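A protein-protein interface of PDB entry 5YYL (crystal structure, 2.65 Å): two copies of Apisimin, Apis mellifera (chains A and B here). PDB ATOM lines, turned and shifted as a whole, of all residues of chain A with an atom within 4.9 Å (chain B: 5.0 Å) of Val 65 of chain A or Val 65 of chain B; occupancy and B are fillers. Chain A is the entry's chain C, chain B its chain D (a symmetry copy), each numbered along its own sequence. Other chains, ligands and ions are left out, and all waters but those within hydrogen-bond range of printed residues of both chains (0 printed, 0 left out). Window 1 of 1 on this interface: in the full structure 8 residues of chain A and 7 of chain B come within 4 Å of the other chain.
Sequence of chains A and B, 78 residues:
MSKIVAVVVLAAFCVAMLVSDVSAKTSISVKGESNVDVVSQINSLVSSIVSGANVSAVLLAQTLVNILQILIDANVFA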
ATOM      1  N   ALA A  61      -1.002  -7.442 -18.473  1.00  0.00           N
ATOM      2  CA  ALA A  61      -1.121  -6.184 -17.724  1.00  0.00           C
ATOM      3  C   ALA A  61       0.177  -5.405 -17.682  1.00  0.00           C
ATOM      4  O   ALA A  61       0.196  -4.199 -17.954  1.00  0.00           O
ATOM      5  CB  ALA A  61      -1.592  -6.449 -16.307  1.00  0.00           C
ATOM      6  N   GLN A  62       1.257  -6.097 -17.342  1.00  0.00           N
ATOM      7  CA  GLN A  62       2.556  -5.456 -17.223  1.00  0.00           C
ATOM      8  C   GLN A  62       3.083  -4.903 -18.549  1.00  0.00           C
ATOM      9  O   GLN A  62       3.719  -3.842 -18.576  1.00  0.00           O
ATOM     10  CB  GLN A  62       3.583  -6.427 -16.643  1.00  0.00           C
ATOM     11  CG  GLN A  62       4.914  -5.783 -16.288  1.00  0.00           C
ATOM     12  CD  GLN A  62       4.763  -4.625 -15.330  1.00  0.00           C
ATOM     13  OE1 GLN A  62       4.515  -4.811 -14.134  1.00  0.00           O
ATOM     14  NE2 GLN A  62       4.890  -3.419 -15.853  1.00  0.00           N
ATOM     15  N   THR A  63       2.839  -5.636 -19.637  1.00  0.00           N
ATOM     16  CA  THR A  63       3.298  -5.209 -20.962  1.00  0.00           C
ATOM     17  C   THR A  63       2.461  -4.035 -21.467  1.00  0.00           C
ATOM     18  O   THR A  63       2.999  -3.125 -22.110  1.00  0.00           O
ATOM     19  CB  THR A  63       3.310  -6.390 -21.968  1.00  0.00           C
ATOM     20  OG1 THR A  63       4.247  -7.369 -21.503  1.00  0.00           O
ATOM     21  CG2 THR A  63       3.733  -5.948 -23.351  1.00  0.00           C
ATOM     22  N   LEU A  64       1.165  -4.046 -21.153  1.00  0.00           N
ATOM     23  CA  LEU A  64       0.302  -2.914 -21.457  1.00  0.00           C
ATOM     24  C   LEU A  64       0.789  -1.676 -20.716  1.00  0.00           C
ATOM     25  O   LEU A  64       0.856  -0.597 -21.292  1.00  0.00           O
ATOM     26  CB  LEU A  64      -1.151  -3.233 -21.095  1.00  0.00           C
ATOM     27  CG  LEU A  64      -2.195  -2.122 -21.285  1.00  0.00           C
ATOM     28  CD1 LEU A  64      -2.048  -1.342 -22.605  1.00  0.00           C
ATOM     29  CD2 LEU A  64      -3.605  -2.708 -21.167  1.00  0.00           C
ATOM     30  N   VAL A  65       1.143  -1.844 -19.445  1.00  0.00           N
ATOM     31  CA  VAL A  65       1.697  -0.750 -18.624  1.00  0.00           C
ATOM     32  C   VAL A  65       2.970  -0.181 -19.225  1.00  0.00           C
ATOM     33  O   VAL A  65       3.147   1.025 -19.241  1.00  0.00           O
ATOM     34  CB  VAL A  65       1.986  -1.225 -17.170  1.00  0.00           C
ATOM     35  CG1 VAL A  65       2.937  -0.283 -16.425  1.00  0.00           C
ATOM     36  CG2 VAL A  65       0.680  -1.421 -16.392  1.00  0.00           C
ATOM     37  N   ASN A  66       3.857  -1.049 -19.699  1.00  0.00           N
ATOM     38  CA  ASN A  66       5.155  -0.618 -20.238  1.00  0.00           C
ATOM     39  C   ASN A  66       5.055   0.024 -21.605  1.00  0.00           C
ATOM     40  O   ASN A  66       5.794   0.961 -21.886  1.00  0.00           O
ATOM     41  CB  ASN A  66       6.144  -1.791 -20.312  1.00  0.00           C
ATOM     42  CG  ASN A  66       6.530  -2.311 -18.952  1.00  0.00           C
ATOM     43  OD1 ASN A  66       6.510  -1.582 -17.969  1.00  0.00           O
ATOM     44  ND2 ASN A  66       6.877  -3.581 -18.891  1.00  0.00           N
ATOM     45  N   ILE A  67       4.174  -0.492 -22.458  1.00  0.00           N
ATOM     46  CA  ILE A  67       3.954   0.108 -23.770  1.00  0.00           C
ATOM     47  C   ILE A  67       3.383   1.501 -23.588  1.00  0.00           C
ATOM     48  O   ILE A  67       3.864   2.436 -24.223  1.00  0.00           O
ATOM     49  CB  ILE A  67       3.013  -0.733 -24.651  1.00  0.00           C
ATOM     50  CG1 ILE A  67       3.732  -2.017 -25.075  1.00  0.00           C
ATOM     51  CG2 ILE A  67       2.556   0.055 -25.884  1.00  0.00           C
ATOM     52  CD1 ILE A  67       2.817  -3.053 -25.664  1.00  0.00           C
ATOM     53  N   LEU A  68       2.372   1.634 -22.726  1.00  0.00           N
ATOM     54  CA  LEU A  68       1.773   2.929 -22.448  1.00  0.00           C
ATOM     55  C   LEU A  68       2.799   3.922 -21.951  1.00  0.00           C
ATOM     56  O   LEU A  68       2.917   5.004 -22.511  1.00  0.00           O
ATOM     57  CB  LEU A  68       0.632   2.810 -21.438  1.00  0.00           C
ATOM     58  CG  LEU A  68      -0.683   2.336 -22.045  1.00  0.00           C
ATOM     59  CD1 LEU A  68      -1.597   1.750 -21.000  1.00  0.00           C
ATOM     60  CD2 LEU A  68      -1.364   3.512 -22.727  1.00  0.00           C
ATOM     61  N   GLN A  69       3.556   3.551 -20.923  1.00  0.00           N
ATOM     62  CA  GLN A  69       4.539   4.467 -20.337  1.00  0.00           C
ATOM     63  C   GLN A  69       5.533   4.945 -21.381  1.00  0.00           C
ATOM     64  O   GLN A  69       5.875   6.120 -21.411  1.00  0.00           O
ATOM     65  CB  GLN A  69       5.304   3.815 -19.187  1.00  0.00           C
ATOM     66  CG  GLN A  69       6.206   4.777 -18.414  1.00  0.00           C
ATOM     67  CD  GLN A  69       5.425   5.909 -17.754  1.00  0.00           C
ATOM     68  OE1 GLN A  69       4.854   5.731 -16.667  1.00  0.00           O
ATOM     69  NE2 GLN A  69       5.383   7.086 -18.422  1.00  0.00           N
ATOM     70  N   ILE A  72       3.689   7.456 -23.421  1.00  0.00           N
ATOM     71  CA  ILE A  72       3.593   8.668 -22.620  1.00  0.00           C
ATOM     72  C   ILE A  72       4.889   9.474 -22.684  1.00  0.00           C
ATOM     73  O   ILE A  72       4.863  10.677 -22.955  1.00  0.00           O
ATOM     74  CB  ILE A  72       3.257   8.349 -21.144  1.00  0.00           C
ATOM     75  CG1 ILE A  72       1.803   7.885 -21.049  1.00  0.00           C
ATOM     76  CG2 ILE A  72       3.515   9.561 -20.233  1.00  0.00           C
ATOM     77  CD1 ILE A  72       1.364   7.437 -19.671  1.00  0.00           C
ATOM     78  N   ALA B  61      -3.655   8.777 -19.163  1.00  0.00           N
ATOM     79  CA  ALA B  61      -2.757   7.658 -19.489  1.00  0.00           C
ATOM     80  C   ALA B  61      -1.808   7.316 -18.355  1.00  0.00           C
ATOM     81  O   ALA B  61      -1.655   6.152 -18.002  1.00  0.00           O
ATOM     82  CB  ALA B  61      -1.955   7.959 -20.741  1.00  0.00           C
ATOM     83  N   GLN B  62      -1.167   8.331 -17.793  1.00  0.00           N
ATOM     84  CA  GLN B  62      -0.221   8.133 -16.691  1.00  0.00           C
ATOM     85  C   GLN B  62      -0.877   7.563 -15.434  1.00  0.00           C
ATOM     86  O   GLN B  62      -0.271   6.750 -14.736  1.00  0.00           O
ATOM     87  CB  GLN B  62       0.475   9.454 -16.341  1.00  0.00           C
ATOM     88  CG  GLN B  62       1.599   9.325 -15.324  1.00  0.00           C
ATOM     89  CD  GLN B  62       2.669   8.343 -15.789  1.00  0.00           C
ATOM     90  OE1 GLN B  62       3.465   8.653 -16.689  1.00  0.00           O
ATOM     91  NE2 GLN B  62       2.669   7.139 -15.205  1.00  0.00           N
ATOM     92  N   THR B  63      -2.092   8.012 -15.128  1.00  0.00           N
ATOM     93  CA  THR B  63      -2.801   7.536 -13.937  1.00  0.00           C
ATOM     94  C   THR B  63      -3.305   6.097 -14.154  1.00  0.00           C
ATOM     95  O   THR B  63      -3.299   5.286 -13.226  1.00  0.00           O
ATOM     96  CB  THR B  63      -3.929   8.491 -13.518  1.00  0.00           C
ATOM     97  OG1 THR B  63      -3.367   9.761 -13.184  1.00  0.00           O
ATOM     98  CG2 THR B  63      -4.682   7.961 -12.292  1.00  0.00           C
ATOM     99  N   LEU B  64      -3.712   5.781 -15.379  1.00  0.00           N
ATOM    100  CA  LEU B  64      -4.051   4.411 -15.752  1.00  0.00           C
ATOM    101  C   LEU B  64      -2.839   3.507 -15.582  1.00  0.00           C
ATOM    102  O   LEU B  64      -2.961   2.419 -15.046  1.00  0.00           O
ATOM    103  CB  LEU B  64      -4.572   4.358 -17.194  1.00  0.00           C
ATOM    104  CG  LEU B  64      -4.835   2.991 -17.846  1.00  0.00           C
ATOM    105  CD1 LEU B  64      -5.657   2.091 -16.930  1.00  0.00           C
ATOM    106  CD2 LEU B  64      -5.501   3.189 -19.201  1.00  0.00           C
ATOM    107  N   VAL B  65      -1.675   3.976 -16.019  1.00  0.00           N
ATOM    108  CA  VAL B  65      -0.409   3.243 -15.859  1.00  0.00           C
ATOM    109  C   VAL B  65      -0.093   2.973 -14.394  1.00  0.00           C
ATOM    110  O   VAL B  65       0.325   1.875 -14.054  1.00  0.00           O
ATOM    111  CB  VAL B  65       0.784   4.009 -16.501  1.00  0.00           C
ATOM    112  CG1 VAL B  65       2.141   3.505 -15.990  1.00  0.00           C
ATOM    113  CG2 VAL B  65       0.709   3.954 -18.028  1.00  0.00           C
ATOM    114  N   ASN B  66      -0.291   3.977 -13.544  1.00  0.00           N
ATOM    115  CA  ASN B  66       0.039   3.861 -12.120  1.00  0.00           C
ATOM    116  C   ASN B  66      -0.939   2.985 -11.344  1.00  0.00           C
ATOM    117  O   ASN B  66      -0.524   2.260 -10.443  1.00  0.00           O
ATOM    118  CB  ASN B  66       0.103   5.242 -11.459  1.00  0.00           C
ATOM    119  CG  ASN B  66       1.241   6.086 -11.981  1.00  0.00           C
ATOM    120  OD1 ASN B  66       2.255   5.558 -12.428  1.00  0.00           O
ATOM    121  ND2 ASN B  66       1.083   7.399 -11.933  1.00  0.00           N
ATOM    122  N   ILE B  67      -2.229   3.079 -11.667  1.00  0.00           N
ATOM    123  CA  ILE B  67      -3.233   2.241 -11.025  1.00  0.00           C
ATOM    124  C   ILE B  67      -2.966   0.784 -11.369  1.00  0.00           C
ATOM    125  O   ILE B  67      -2.965  -0.071 -10.480  1.00  0.00           O
ATOM    126  CB  ILE B  67      -4.668   2.613 -11.427  1.00  0.00           C
ATOM    127  CG1 ILE B  67      -5.043   3.969 -10.830  1.00  0.00           C
ATOM    128  CG2 ILE B  67      -5.659   1.559 -10.926  1.00  0.00           C
ATOM    129  CD1 ILE B  67      -6.286   4.587 -11.429  1.00  0.00           C
ATOM    130  N   LEU B  68      -2.736   0.516 -12.651  1.00  0.00           N
ATOM    131  CA  LEU B  68      -2.444  -0.840 -13.104  1.00  0.00           C
ATOM    132  C   LEU B  68      -1.220  -1.411 -12.398  1.00  0.00           C
ATOM    133  O   LEU B  68      -1.291  -2.485 -11.823  1.00  0.00           O
ATOM    134  CB  LEU B  68      -2.239  -0.891 -14.613  1.00  0.00           C
ATOM    135  CG  LEU B  68      -3.540  -0.879 -15.408  1.00  0.00           C
ATOM    136  CD1 LEU B  68      -3.257  -0.470 -16.847  1.00  0.00           C
ATOM    137  CD2 LEU B  68      -4.271  -2.216 -15.344  1.00  0.00           C
ATOM    138  N   GLN B  69      -0.118  -0.672 -12.412  1.00  0.00           N
ATOM    139  CA  GLN B  69       1.114  -1.161 -11.802  1.00  0.00           C
ATOM    140  C   GLN B  69       0.919  -1.496 -10.334  1.00  0.00           C
ATOM    141  O   GLN B  69       1.413  -2.514  -9.857  1.00  0.00           O
ATOM    142  CB  GLN B  69       2.250  -0.151 -11.945  1.00  0.00           C
ATOM    143  CG  GLN B  69       3.612  -0.701 -11.524  1.00  0.00           C
ATOM    144  CD  GLN B  69       4.057  -1.901 -12.354  1.00  0.00           C
ATOM    145  OE1 GLN B  69       4.548  -1.756 -13.493  1.00  0.00           O
ATOM    146  NE2 GLN B  69       3.874  -3.093 -11.795  1.00  0.00           N
ATOM    147  N   ILE B  72      -0.920  -4.725 -10.310  1.00  0.00           N
ATOM    148  CA  ILE B  72       0.045  -5.769 -10.649  1.00  0.00           C
ATOM    149  C   ILE B  72       0.880  -6.171  -9.434  1.00  0.00           C
ATOM    150  O   ILE B  72       1.005  -7.350  -9.117  1.00  0.00           O
ATOM    151  CB  ILE B  72       0.967  -5.327 -11.798  1.00  0.00           C
ATOM    152  CG1 ILE B  72       0.165  -5.299 -13.112  1.00  0.00           C
ATOM    153  CG2 ILE B  72       2.188  -6.245 -11.916  1.00  0.00           C
ATOM    154  CD1 ILE B  72       0.937  -4.786 -14.312  1.00  0.00           C
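Printed residues of chain B within 4 Å of Ala 61 of chain A: Ile 72 (3.5 Å).
Of chain B, only Val 65 (3.9 Å), Leu 68 (3.5 Å), Gln 69 (3.7 Å) and Ile 72 (3.96 Å) come within 4 Å of Val 65 of chain A.
Printed residues of chain B within 4 Å of Leu 68 of chain A: Val 65 (3.6 Å).
Of the printed residues of chain B, Gln 69 of chain A touches Gln 62 (3.0 Å) and Val 65 (3.6 Å).
Printed residues of chain B within 4 Å of Ile 72 of chain A: Ala 61 (3.4 Å), Gln 62 (3.3 Å) and Val 65 (3.9 Å).
Leu 64 of chain B touches none of the printed residues of chain A.
Of chain A, only Val 65 (3.9 Å), Leu 68 (3.6 Å), Gln 69 (3.6 Å) and Ile 72 (3.9 Å) come within 4 Å of Val 65 of chain B.
Printed residues of chain A within 4 Å of Gln 69 of chain B: Gln 62 (2.9 Å) and Val 65 (3.7 Å).
The nearest printed residue of chain B that does not touch Val 65 of chain A is Leu 64 of chain B (5.5 Å).
The nearest printed residue of chain A that does not touch Val 65 of chain B is Leu 64 of chain A (5.6 Å).
The nearest printed residue of chain A that does not touch Leu 68 of chain B is Leu 64 of chain A (4.9 Å).
Among the printed residues, merely in contact across the chains: Ala 61 of chain A with Ile 72 of chain B (3.5 Å), Gln 62 of chain A with Ile 72 of chain B (3.3 Å), Val 65 of chain A with Val 65 of chain B (3.9 Å), Val 65 of chain A with Leu 68 of chain B (3.5 Å), Val 65 of chain A with Gln 69 of chain B (3.7 Å), Val 65 of chain A with Ile 72 of chain B (3.96 Å), Leu 68 of chain A with Val 65 of chain B (3.6 Å), Gln 69 of chain A with Val 65 of chain B (3.6 Å), Ile 72 of chain A with Ala 61 of chain B (3.4 Å), Ile 72 of chain A with Gln 62 of chain B (3.3 Å) and Ile 72 of chain A with Val 65 of chain B (3.9 Å).
The backbone carbonyl oxygen (O) of Gln 62 of chain A is in hydrogen-bond range of the side-chain amide nitrogen (ND2) of Asn 66 of chain A.
ND2 of Asn 66 of chain B sits at hydrogen-bond distance from O of Gln 62 of chain B, at 3.2 Å.
Gln 62 of chain A touches Ile 72 of chain B, and with the chains exchanged Ile 72 of chain A touches Gln 62 of chain B.
Val 65 of chain B touches its own counterpart, Val 65 of chain A.
Val 65 of chain A touches Leu 68 of chain B, and with the chains exchanged Leu 68 of chain A touches Val 65 of chain B.
Val 65 of chain A touches Gln 69 of chain B, and with the chains exchanged Gln 69 of chain A touches Val 65 of chain B.
NE2 of Gln 62 of chain B lies within hydrogen-bond range of OE1 of Gln 69 of chain A, at 3.0 Å.
NE2 of Gln 62 of chain A lies within hydrogen-bond range of OE1 of Gln 69 of chain B, 2.9 Å away.
Of the 10 printed residues of chain B, 6 touch a printed residue of chain A.
Printed residues of chain B that touch a printed residue of chain A: Ala 61, Gln 62, Val 65, Leu 68, Gln 69 and Ile 72.
Hydrophobic or aromatic side chains of chain B within 4 Å of the printed part of chain A: Ala 61, Val 65, Leu 68 and Ile 72.
Of the 10 printed residues of chain A, 6 touch a printed residue of chain B.
Printed residues of chain A that touch a printed residue of chain B: Ala 61, Gln 62, Val 65, Leu 68, Gln 69 and Ile 72.
Among the printed residues, 13 pairs touch across the chains.
Among the printed residues, no Asp or Glu carboxylate lies within 4 Å of a Lys or Arg side-chain nitrogen of the other chain.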
